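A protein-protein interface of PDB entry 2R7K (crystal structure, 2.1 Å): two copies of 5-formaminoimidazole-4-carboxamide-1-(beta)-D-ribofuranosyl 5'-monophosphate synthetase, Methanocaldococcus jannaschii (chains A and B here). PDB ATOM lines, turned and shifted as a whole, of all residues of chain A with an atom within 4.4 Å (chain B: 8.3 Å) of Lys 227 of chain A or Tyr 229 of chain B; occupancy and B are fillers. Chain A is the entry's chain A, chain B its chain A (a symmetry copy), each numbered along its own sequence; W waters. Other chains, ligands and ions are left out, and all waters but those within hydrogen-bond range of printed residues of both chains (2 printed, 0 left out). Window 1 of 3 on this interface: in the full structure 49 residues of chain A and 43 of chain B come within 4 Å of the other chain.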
ATOM      1  N   THR A 205     -27.435   2.159  32.437  1.00  0.00           N
ATOM      2  CA  THR A 205     -26.317   2.783  31.749  1.00  0.00           C
ATOM      3  C   THR A 205     -25.301   3.328  32.758  1.00  0.00           C
ATOM      4  O   THR A 205     -25.670   3.953  33.748  1.00  0.00           O
ATOM      5  CB  THR A 205     -26.826   3.896  30.825  1.00  0.00           C
ATOM      6  OG1 THR A 205     -27.915   4.575  31.457  1.00  0.00           O
ATOM      7  CG2 THR A 205     -27.330   3.313  29.523  1.00  0.00           C
ATOM      8  N   ASN A 206     -24.026   3.059  32.510  1.00  0.00           N
ATOM      9  CA  ASN A 206     -22.945   3.487  33.380  1.00  0.00           C
ATOM     10  C   ASN A 206     -22.590   4.971  33.240  1.00  0.00           C
ATOM     11  O   ASN A 206     -22.230   5.441  32.158  1.00  0.00           O
ATOM     12  CB  ASN A 206     -21.700   2.657  33.078  1.00  0.00           C
ATOM     13  CG  ASN A 206     -20.540   2.963  34.015  1.00  0.00           C
ATOM     14  OD1 ASN A 206     -19.386   2.846  33.621  1.00  0.00           O
ATOM     15  ND2 ASN A 206     -20.841   3.323  35.262  1.00  0.00           N
ATOM     16  N   PHE A 207     -22.694   5.700  34.343  1.00  0.00           N
ATOM     17  CA  PHE A 207     -22.142   7.054  34.431  1.00  0.00           C
ATOM     18  C   PHE A 207     -21.236   7.132  35.646  1.00  0.00           C
ATOM     19  O   PHE A 207     -21.709   7.081  36.778  1.00  0.00           O
ATOM     20  CB  PHE A 207     -23.254   8.083  34.568  1.00  0.00           C
ATOM     21  CG  PHE A 207     -24.198   8.108  33.404  1.00  0.00           C
ATOM     22  CD1 PHE A 207     -23.953   8.924  32.313  1.00  0.00           C
ATOM     23  CD2 PHE A 207     -25.337   7.317  33.402  1.00  0.00           C
ATOM     24  CE1 PHE A 207     -24.828   8.955  31.241  1.00  0.00           C
ATOM     25  CE2 PHE A 207     -26.209   7.338  32.325  1.00  0.00           C
ATOM     26  CZ  PHE A 207     -25.951   8.163  31.243  1.00  0.00           C
ATOM     27  N   ASP A 226     -17.585   9.566  32.526  1.00  0.00           N
ATOM     28  CA  ASP A 226     -17.182   8.499  31.608  1.00  0.00           C
ATOM     29  C   ASP A 226     -17.976   7.217  31.877  1.00  0.00           C
ATOM     30  O   ASP A 226     -18.598   7.065  32.928  1.00  0.00           O
ATOM     31  CB  ASP A 226     -15.681   8.185  31.748  1.00  0.00           C
ATOM     32  CG  ASP A 226     -15.344   7.443  33.055  1.00  0.00           C
ATOM     33  OD1 ASP A 226     -15.343   8.097  34.118  1.00  0.00           O
ATOM     34  OD2 ASP A 226     -15.043   6.215  33.024  1.00  0.00           O
ATOM     35  N   LYS A 227     -17.946   6.297  30.918  1.00  0.00           N
ATOM     36  CA  LYS A 227     -18.377   4.928  31.168  1.00  0.00           C
ATOM     37  C   LYS A 227     -17.158   4.016  31.083  1.00  0.00           C
ATOM     38  O   LYS A 227     -16.234   4.264  30.310  1.00  0.00           O
ATOM     39  CB  LYS A 227     -19.475   4.491  30.194  1.00  0.00           C
ATOM     40  CG  LYS A 227     -19.009   4.136  28.791  1.00  0.00           C
ATOM     41  CD  LYS A 227     -20.183   3.645  27.931  1.00  0.00           C
ATOM     42  CE  LYS A 227     -19.711   2.675  26.859  1.00  0.00           C
ATOM     43  NZ  LYS A 227     -20.832   2.058  26.102  1.00  0.00           N
ATOM     44  N   ARG A 228     -17.153   2.971  31.895  1.00  0.00           N
ATOM     45  CA  ARG A 228     -16.015   2.072  31.975  1.00  0.00           C
ATOM     46  C   ARG A 228     -15.972   1.200  30.741  1.00  0.00           C
ATOM     47  O   ARG A 228     -17.011   0.914  30.132  1.00  0.00           O
ATOM     48  CB  ARG A 228     -16.119   1.183  33.218  1.00  0.00           C
ATOM     49  CG  ARG A 228     -16.146   1.944  34.524  1.00  0.00           C
ATOM     50  CD  ARG A 228     -14.809   2.613  34.774  1.00  0.00           C
ATOM     51  NE  ARG A 228     -14.610   2.905  36.189  1.00  0.00           N
ATOM     52  CZ  ARG A 228     -14.369   4.115  36.687  1.00  0.00           C
ATOM     53  NH1 ARG A 228     -14.279   5.168  35.887  1.00  0.00           N
ATOM     54  NH2 ARG A 228     -14.208   4.265  37.995  1.00  0.00           N
ATOM     55  N   TYR A 229     -14.759   0.797  30.376  1.00  0.00           N
ATOM     56  CA  TYR A 229     -14.514  -0.086  29.252  1.00  0.00           C
ATOM     57  C   TYR A 229     -13.723  -1.230  29.855  1.00  0.00           C
ATOM     58  O   TYR A 229     -12.533  -1.083  30.149  1.00  0.00           O
ATOM     59  CB  TYR A 229     -13.693   0.653  28.193  1.00  0.00           C
ATOM     60  CG  TYR A 229     -13.734   0.069  26.816  1.00  0.00           C
ATOM     61  CD1 TYR A 229     -14.887  -0.520  26.325  1.00  0.00           C
ATOM     62  CD2 TYR A 229     -12.626   0.142  25.980  1.00  0.00           C
ATOM     63  CE1 TYR A 229     -14.930  -1.038  25.049  1.00  0.00           C
ATOM     64  CE2 TYR A 229     -12.665  -0.367  24.699  1.00  0.00           C
ATOM     65  CZ  TYR A 229     -13.820  -0.960  24.244  1.00  0.00           C
ATOM     66  OH  TYR A 229     -13.868  -1.488  22.973  1.00  0.00           O
ATOM     67  N   ASN A 258     -11.689   3.983  29.272  1.00  0.00           N
ATOM     68  CA  ASN A 258     -12.900   4.758  29.480  1.00  0.00           C
ATOM     69  C   ASN A 258     -13.376   5.422  28.205  1.00  0.00           C
ATOM     70  O   ASN A 258     -12.596   5.699  27.290  1.00  0.00           O
ATOM     71  CB  ASN A 258     -12.696   5.823  30.578  1.00  0.00           C
ATOM     72  CG  ASN A 258     -11.884   5.310  31.758  1.00  0.00           C
ATOM     73  OD1 ASN A 258     -12.429   5.028  32.831  1.00  0.00           O
ATOM     74  ND2 ASN A 258     -10.578   5.189  31.570  1.00  0.00           N
ATOM     75  N   ILE A 259     -14.678   5.668  28.154  1.00  0.00           N
ATOM     76  CA  ILE A 259     -15.330   6.242  26.995  1.00  0.00           C
ATOM     77  C   ILE A 259     -16.098   7.439  27.533  1.00  0.00           C
ATOM     78  O   ILE A 259     -16.711   7.341  28.593  1.00  0.00           O
ATOM     79  CB  ILE A 259     -16.290   5.212  26.355  1.00  0.00           C
ATOM     80  CG1 ILE A 259     -15.499   3.993  25.862  1.00  0.00           C
ATOM     81  CG2 ILE A 259     -17.088   5.824  25.219  1.00  0.00           C
ATOM     82  CD1 ILE A 259     -16.363   2.801  25.494  1.00  0.00           C
ATOM     83  N   VAL A 261     -19.030  10.193  27.987  1.00  0.00           N
ATOM     84  CA  VAL A 261     -20.470  10.153  27.892  1.00  0.00           C
ATOM     85  C   VAL A 261     -20.992  11.420  28.548  1.00  0.00           C
ATOM     86  O   VAL A 261     -20.334  11.987  29.409  1.00  0.00           O
ATOM     87  CB  VAL A 261     -21.039   8.903  28.633  1.00  0.00           C
ATOM     88  CG1 VAL A 261     -20.860   9.038  30.145  1.00  0.00           C
ATOM     89  CG2 VAL A 261     -22.501   8.694  28.288  1.00  0.00           C
ATOM     90  N   ASN B 206     -25.850   3.316  15.271  1.00  0.00           N
ATOM     91  CA  ASN B 206     -26.573   4.556  15.493  1.00  0.00           C
ATOM     92  C   ASN B 206     -25.737   5.814  15.234  1.00  0.00           C
ATOM     93  O   ASN B 206     -24.697   6.027  15.860  1.00  0.00           O
ATOM     94  CB  ASN B 206     -27.076   4.592  16.934  1.00  0.00           C
ATOM     95  CG  ASN B 206     -27.939   5.809  17.232  1.00  0.00           C
ATOM     96  OD1 ASN B 206     -27.959   6.287  18.361  1.00  0.00           O
ATOM     97  ND2 ASN B 206     -28.676   6.295  16.235  1.00  0.00           N
ATOM     98  N   CYS B 208     -26.894   9.743  15.289  1.00  0.00           N
ATOM     99  CA  CYS B 208     -27.800  10.879  15.372  1.00  0.00           C
ATOM    100  C   CYS B 208     -27.060  12.100  14.827  1.00  0.00           C
ATOM    101  O   CYS B 208     -26.167  12.635  15.465  1.00  0.00           O
ATOM    102  CB  CYS B 208     -28.258  11.092  16.812  1.00  0.00           C
ATOM    103  SG  CYS B 208     -28.977   9.574  17.563  1.00  0.00           S
ATOM    104  N   ASP B 226     -23.850  11.951  17.568  1.00  0.00           N
ATOM    105  CA  ASP B 226     -23.786  11.113  18.767  1.00  0.00           C
ATOM    106  C   ASP B 226     -24.512   9.783  18.543  1.00  0.00           C
ATOM    107  O   ASP B 226     -25.293   9.637  17.603  1.00  0.00           O
ATOM    108  CB  ASP B 226     -24.426  11.823  19.974  1.00  0.00           C
ATOM    109  CG  ASP B 226     -25.961  11.897  19.882  1.00  0.00           C
ATOM    110  OD1 ASP B 226     -26.461  12.720  19.088  1.00  0.00           O
ATOM    111  OD2 ASP B 226     -26.675  11.164  20.625  1.00  0.00           O
ATOM    112  N   LYS B 227     -24.246   8.816  19.417  1.00  0.00           N
ATOM    113  CA  LYS B 227     -25.091   7.632  19.515  1.00  0.00           C
ATOM    114  C   LYS B 227     -25.806   7.662  20.861  1.00  0.00           C
ATOM    115  O   LYS B 227     -25.267   8.148  21.854  1.00  0.00           O
ATOM    116  CB  LYS B 227     -24.284   6.343  19.335  1.00  0.00           C
ATOM    117  CG  LYS B 227     -23.457   5.910  20.536  1.00  0.00           C
ATOM    118  CD  LYS B 227     -22.754   4.572  20.264  1.00  0.00           C
ATOM    119  CE  LYS B 227     -22.529   3.796  21.552  1.00  0.00           C
ATOM    120  NZ  LYS B 227     -21.990   2.430  21.319  1.00  0.00           N
ATOM    121  N   ARG B 228     -27.029   7.156  20.882  1.00  0.00           N
ATOM    122  CA  ARG B 228     -27.852   7.201  22.078  1.00  0.00           C
ATOM    123  C   ARG B 228     -27.342   6.188  23.080  1.00  0.00           C
ATOM    124  O   ARG B 228     -26.762   5.163  22.703  1.00  0.00           O
ATOM    125  CB  ARG B 228     -29.312   6.883  21.739  1.00  0.00           C
ATOM    126  CG  ARG B 228     -29.943   7.847  20.759  1.00  0.00           C
ATOM    127  CD  ARG B 228     -30.097   9.216  21.389  1.00  0.00           C
ATOM    128  NE  ARG B 228     -31.125  10.004  20.717  1.00  0.00           N
ATOM    129  CZ  ARG B 228     -30.925  11.198  20.165  1.00  0.00           C
ATOM    130  NH1 ARG B 228     -29.729  11.769  20.206  1.00  0.00           N
ATOM    131  NH2 ARG B 228     -31.935  11.823  19.575  1.00  0.00           N
ATOM    132  N   TYR B 229     -27.555   6.499  24.355  1.00  0.00           N
ATOM    133  CA  TYR B 229     -27.188   5.636  25.461  1.00  0.00           C
ATOM    134  C   TYR B 229     -28.482   5.460  26.229  1.00  0.00           C
ATOM    135  O   TYR B 229     -28.922   6.372  26.936  1.00  0.00           O
ATOM    136  CB  TYR B 229     -26.128   6.329  26.320  1.00  0.00           C
ATOM    137  CG  TYR B 229     -25.327   5.433  27.211  1.00  0.00           C
ATOM    138  CD1 TYR B 229     -24.978   4.154  26.809  1.00  0.00           C
ATOM    139  CD2 TYR B 229     -24.876   5.880  28.446  1.00  0.00           C
ATOM    140  CE1 TYR B 229     -24.222   3.338  27.622  1.00  0.00           C
ATOM    141  CE2 TYR B 229     -24.112   5.071  29.262  1.00  0.00           C
ATOM    142  CZ  TYR B 229     -23.795   3.801  28.843  1.00  0.00           C
ATOM    143  OH  TYR B 229     -23.047   2.975  29.653  1.00  0.00           O
ATOM    144  N   GLU B 230     -29.104   4.292  26.069  1.00  0.00           N
ATOM    145  CA  GLU B 230     -30.480   4.065  26.522  1.00  0.00           C
ATOM    146  C   GLU B 230     -30.581   2.970  27.592  1.00  0.00           C
ATOM    147  O   GLU B 230     -29.844   1.998  27.560  1.00  0.00           O
ATOM    148  CB  GLU B 230     -31.369   3.740  25.315  1.00  0.00           C
ATOM    149  CG  GLU B 230     -31.624   4.940  24.415  1.00  0.00           C
ATOM    150  CD  GLU B 230     -32.032   4.570  23.004  1.00  0.00           C
ATOM    151  OE1 GLU B 230     -31.728   3.445  22.557  1.00  0.00           O
ATOM    152  OE2 GLU B 230     -32.656   5.420  22.333  1.00  0.00           O
ATOM    153  N   SER B 231     -31.490   3.149  28.546  1.00  0.00           N
ATOM    154  CA  SER B 231     -31.701   2.182  29.623  1.00  0.00           C
ATOM    155  C   SER B 231     -33.135   1.631  29.530  1.00  0.00           C
ATOM    156  O   SER B 231     -34.071   2.396  29.320  1.00  0.00           O
ATOM    157  CB  SER B 231     -31.469   2.863  30.973  1.00  0.00           C
ATOM    158  OG  SER B 231     -31.476   1.941  32.050  1.00  0.00           O
ATOM    159  N   ASN B 232     -33.328   0.323  29.721  1.00  0.00           N
ATOM    160  CA  ASN B 232     -32.308  -0.592  30.235  1.00  0.00           C
ATOM    161  C   ASN B 232     -31.514  -1.288  29.144  1.00  0.00           C
ATOM    162  O   ASN B 232     -30.581  -2.033  29.422  1.00  0.00           O
ATOM    163  CB  ASN B 232     -32.964  -1.643  31.145  1.00  0.00           C
ATOM    164  CG  ASN B 232     -33.847  -2.627  30.374  1.00  0.00           C
ATOM    165  OD1 ASN B 232     -33.793  -2.711  29.146  1.00  0.00           O
ATOM    166  ND2 ASN B 232     -34.658  -3.382  31.102  1.00  0.00           N
ATOM    167  N   ILE B 233     -31.868  -1.028  27.894  1.00  0.00           N
ATOM    168  CA  ILE B 233     -31.350  -1.831  26.793  1.00  0.00           C
ATOM    169  C   ILE B 233     -29.818  -1.926  26.765  1.00  0.00           C
ATOM    170  O   ILE B 233     -29.264  -3.016  26.596  1.00  0.00           O
ATOM    171  CB  ILE B 233     -31.914  -1.354  25.434  1.00  0.00           C
ATOM    172  CG1 ILE B 233     -31.446  -2.278  24.301  1.00  0.00           C
ATOM    173  CG2 ILE B 233     -31.551   0.104  25.170  1.00  0.00           C
ATOM    174  CD1 ILE B 233     -31.887  -3.735  24.478  1.00  0.00           C
ATOM    175  N   ASP B 234     -29.130  -0.797  26.942  1.00  0.00           N
ATOM    176  CA  ASP B 234     -27.668  -0.796  26.871  1.00  0.00           C
ATOM    177  C   ASP B 234     -27.036  -1.422  28.121  1.00  0.00           C
ATOM    178  O   ASP B 234     -25.869  -1.817  28.112  1.00  0.00           O
ATOM    179  CB  ASP B 234     -27.132   0.611  26.569  1.00  0.00           C
ATOM    180  CG  ASP B 234     -27.414   1.037  25.136  1.00  0.00           C
ATOM    181  OD1 ASP B 234     -27.215   0.201  24.221  1.00  0.00           O
ATOM    182  OD2 ASP B 234     -27.844   2.191  24.911  1.00  0.00           O
ATOM    183  N   GLY B 235     -27.821  -1.534  29.184  1.00  0.00           N
ATOM    184  CA  GLY B 235     -27.441  -2.369  30.328  1.00  0.00           C
ATOM    185  C   GLY B 235     -27.777  -3.842  30.098  1.00  0.00           C
ATOM    186  O   GLY B 235     -27.000  -4.723  30.463  1.00  0.00           O
ATOM    187  N   ARG B 238     -25.446  -5.847  27.945  1.00  0.00           N
ATOM    188  CA  ARG B 238     -24.121  -5.942  28.542  1.00  0.00           C
ATOM    189  C   ARG B 238     -24.055  -7.131  29.498  1.00  0.00           C
ATOM    190  O   ARG B 238     -23.027  -7.379  30.130  1.00  0.00           O
ATOM    191  CB  ARG B 238     -23.755  -4.652  29.283  1.00  0.00           C
ATOM    192  CG  ARG B 238     -22.261  -4.350  29.251  1.00  0.00           C
ATOM    193  CD  ARG B 238     -21.778  -3.807  30.564  1.00  0.00           C
ATOM    194  NE  ARG B 238     -20.343  -3.532  30.543  1.00  0.00           N
ATOM    195  CZ  ARG B 238     -19.581  -3.484  31.629  1.00  0.00           C
ATOM    196  NH1 ARG B 238     -20.111  -3.711  32.821  1.00  0.00           N
ATOM    197  NH2 ARG B 238     -18.287  -3.212  31.521  1.00  0.00           N
ATOM    198  N   SER B 252     -36.164  -1.898  27.642  1.00  0.00           N
ATOM    199  CA  SER B 252     -36.732  -0.562  27.512  1.00  0.00           C
ATOM    200  C   SER B 252     -35.692   0.357  26.870  1.00  0.00           C
ATOM    201  O   SER B 252     -34.503   0.045  26.856  1.00  0.00           O
ATOM    202  CB  SER B 252     -37.174  -0.027  28.870  1.00  0.00           C
ATOM    203  OG  SER B 252     -36.166  -0.233  29.838  1.00  0.00           O
ATOM    204  N   TYR B 253     -36.147   1.477  26.328  1.00  0.00           N
ATOM    205  CA  TYR B 253     -35.287   2.353  25.540  1.00  0.00           C
ATOM    206  C   TYR B 253     -35.385   3.805  25.995  1.00  0.00           C
ATOM    207  O   TYR B 253     -35.577   4.709  25.185  1.00  0.00           O
ATOM    208  CB  TYR B 253     -35.654   2.236  24.063  1.00  0.00           C
ATOM    209  CG  TYR B 253     -35.417   0.851  23.500  1.00  0.00           C
ATOM    210  CD1 TYR B 253     -34.271   0.570  22.764  1.00  0.00           C
ATOM    211  CD2 TYR B 253     -36.336  -0.182  23.711  1.00  0.00           C
ATOM    212  CE1 TYR B 253     -34.044  -0.689  22.240  1.00  0.00           C
ATOM    213  CE2 TYR B 253     -36.109  -1.460  23.201  1.00  0.00           C
ATOM    214  CZ  TYR B 253     -34.964  -1.703  22.462  1.00  0.00           C
ATOM    215  OH  TYR B 253     -34.728  -2.960  21.943  1.00  0.00           O
ATOM    216  N   VAL B 254     -35.261   4.015  27.297  1.00  0.00           N
ATOM    217  CA  VAL B 254     -35.303   5.354  27.867  1.00  0.00           C
ATOM    218  C   VAL B 254     -33.973   6.067  27.624  1.00  0.00           C
ATOM    219  O   VAL B 254     -32.914   5.572  28.031  1.00  0.00           O
ATOM    220  CB  VAL B 254     -35.535   5.297  29.381  1.00  0.00           C
ATOM    221  CG1 VAL B 254     -35.806   6.704  29.936  1.00  0.00           C
ATOM    222  CG2 VAL B 254     -36.686   4.351  29.712  1.00  0.00           C
ATOM    223  N   ILE B 255     -34.024   7.222  26.959  1.00  0.00           N
ATOM    224  CA  ILE B 255     -32.814   8.004  26.720  1.00  0.00           C
ATOM    225  C   ILE B 255     -32.202   8.462  28.034  1.00  0.00           C
ATOM    226  O   ILE B 255     -32.852   9.161  28.813  1.00  0.00           O
ATOM    227  CB  ILE B 255     -33.050   9.230  25.795  1.00  0.00           C
ATOM    228  CG1 ILE B 255     -31.717   9.914  25.504  1.00  0.00           C
ATOM    229  CG2 ILE B 255     -34.034  10.223  26.416  1.00  0.00           C
ATOM    230  CD1 ILE B 255     -30.770   9.030  24.717  1.00  0.00           C
ATOM    231  N   THR B 256     -30.963   8.045  28.294  1.00  0.00           N
ATOM    232  CA  THR B 256     -30.276   8.476  29.510  1.00  0.00           C
ATOM    233  C   THR B 256     -29.046   9.348  29.240  1.00  0.00           C
ATOM    234  O   THR B 256     -28.562  10.027  30.138  1.00  0.00           O
ATOM    235  CB  THR B 256     -29.845   7.299  30.427  1.00  0.00           C
ATOM    236  OG1 THR B 256     -28.784   6.550  29.813  1.00  0.00           O
ATOM    237  CG2 THR B 256     -31.019   6.388  30.753  1.00  0.00           C
ATOM    238  N   GLY B 257     -28.538   9.323  28.015  1.00  0.00           N
ATOM    239  CA  GLY B 257     -27.296  10.020  27.718  1.00  0.00           C
ATOM    240  C   GLY B 257     -26.850   9.813  26.290  1.00  0.00           C
ATOM    241  O   GLY B 257     -27.573   9.222  25.490  1.00  0.00           O
ATOM    242  N   ASN B 258     -25.661  10.320  25.969  1.00  0.00           N
ATOM    243  CA  ASN B 258     -25.121  10.234  24.624  1.00  0.00           C
ATOM    244  C   ASN B 258     -23.620  10.029  24.627  1.00  0.00           C
ATOM    245  O   ASN B 258     -22.917  10.405  25.569  1.00  0.00           O
ATOM    246  CB  ASN B 258     -25.473  11.491  23.802  1.00  0.00           C
ATOM    247  CG  ASN B 258     -26.895  11.977  24.043  1.00  0.00           C
ATOM    248  OD1 ASN B 258     -27.784  11.789  23.205  1.00  0.00           O
ATOM    249  ND2 ASN B 258     -27.119  12.607  25.187  1.00  0.00           N
ATOM    250  N   ILE B 259     -23.138   9.417  23.554  1.00  0.00           N
ATOM    251  CA  ILE B 259     -21.738   9.078  23.400  1.00  0.00           C
ATOM    252  C   ILE B 259     -21.338   9.672  22.058  1.00  0.00           C
ATOM    253  O   ILE B 259     -22.100   9.574  21.100  1.00  0.00           O
ATOM    254  CB  ILE B 259     -21.554   7.542  23.399  1.00  0.00           C
ATOM    255  CG1 ILE B 259     -22.008   6.959  24.745  1.00  0.00           C
ATOM    256  CG2 ILE B 259     -20.118   7.151  23.106  1.00  0.00           C
ATOM    257  CD1 ILE B 259     -22.154   5.449  24.748  1.00  0.00           C
HETATM  258  O   HOH W   1     -23.064   1.882  24.583  1.00  0.00           O
HETATM  259  O   HOH W   2     -19.496   3.098  23.314  1.00  0.00           O
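The side-chain hydroxyl of Thr 205 of chain A lies within hydrogen-bond range of the side-chain hydroxyl of Thr 256 of chain B, at 2.7 Å. The backbone NH of Asn 206 of chain A is in hydrogen-bond range of the side-chain hydroxyl of Tyr 229 of chain B.
OD1 of Asn 206 of chain A lies within hydrogen-bond range of N of Arg 228 of chain A, 2.8 Å away. The backbone NH of Lys 227 of chain A sits at hydrogen-bond distance from the backbone carbonyl oxygen of Ile 259 of chain A (2.8 Å). The side-chain amide oxygen of Asn 258 of chain B lies close to the side-chain carboxylate of Asp 226 of chain B (2.9 Å). The backbone carbonyl oxygen (O) of Ile 259 of chain B lies within hydrogen-bond range of the backbone NH (N) of Lys 227 of chain B (2.8 Å). The backbone carbonyl oxygen (O) of Tyr 229 of chain B is in hydrogen-bond range of the side-chain hydroxyl (OG1) of Thr 256 of chain B, at 2.9 Å. The backbone NH (N) of Tyr 229 of chain B sits at hydrogen-bond distance from the backbone carbonyl oxygen (O) of Gly 257 of chain B, 3.0 Å away.
Among the printed residues, pairs that only touch across the chains: Thr 205 of chain A with Tyr 229 of chain B (3.3 Å), Thr 205 of chain A with Glu 230 of chain B (3.5 Å), Thr 205 of chain A with Ser 231 of chain B (3.97 Å), Phe 207 of chain A with Tyr 229 of chain B (3.8 Å), Phe 207 of chain A with Thr 256 of chain B (3.4 Å), Lys 227 of chain A with Tyr 229 of chain B (3.4 Å), Lys 227 of chain A with Ile 259 of chain B (3.9 Å), Ile 259 of chain A with Ile 259 of chain B (3.9 Å), Val 261 of chain A with Tyr 229 of chain B (3.7 Å), Val 261 of chain A with Asn 258 of chain B (3.2 Å) and Val 261 of chain A with Ile 259 of chain B (3.98 Å).
Of the printed residues of chain B, Phe 207 of chain A touches Tyr 229 and Thr 256. Printed residues of chain B within 4 Å of Ile 259 of chain A: Ile 259 (3.9 Å). Of the printed residues of chain B, Val 261 of chain A touches Tyr 229, Asn 258 and Ile 259. Of chain A, only Thr 205 (3.3 Å), Asn 206 (3.0 Å), Phe 207 (3.8 Å), Lys 227 (3.4 Å) and Val 261 (3.7 Å) come within 4 Å of Tyr 229 of chain B. Printed residues of chain A within 4 Å of Glu 230 of chain B: Thr 205 (3.5 Å). Of the printed residues of chain A, Asn 258 of chain B touches Val 261. The nearest residue of chain B that does not touch Lys 227 of chain A is Lys 227 of chain B (4.9 Å). The nearest printed residue of chain A that does not touch Tyr 229 of chain B is Arg 228 of chain A (6.3 Å). The nearest printed residue of chain B that does not touch Thr 205 of chain A is Asp 234 of chain B (4.01 Å).
Along chain B the printed residues that touch a printed residue of chain A span positions 229 to 259. Printed residues of chain A that touch a printed residue of chain B: Thr 205, Asn 206, Phe 207, Lys 227, Ile 259 and Val 261. Hydrophobic or aromatic side chains of chain A that line the printed part of chain B: Phe 207, Ile 259 and Val 261. Among the printed residues, 13 pairs touch across the chains. Among the printed residues, no Asp or Glu carboxylate lies within 4 Å of a Lys or Arg side-chain nitrogen of the other chain.
Asn 206 of chain A touches Tyr 229 of chain B, but with the chains exchanged Tyr 229 of chain A does not touch Asn 206 of chain B (15.0 Å). Lys 227 of chain A touches Tyr 229 of chain B, but with the chains exchanged Tyr 229 of chain A does not touch Lys 227 of chain B (8.7 Å). Lys 227 of chain A touches Ile 259 of chain B, but with the chains exchanged Ile 259 of chain A does not touch Lys 227 of chain B (6.9 Å). Ile 259 of chain B touches its own counterpart, Ile 259 of chain A. Positions printed for both chains: 206, 226, 227, 228, 229, 258 and 259.
Water W1 bridges NZ of Lys 227 of chain A (2.7 Å) and NZ of Lys 227 of chain B (3.5 Å). Water W2 bridges the side-chain amino group of Lys 227 of chain A and the side-chain amino group of Lys 227 of chain B.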
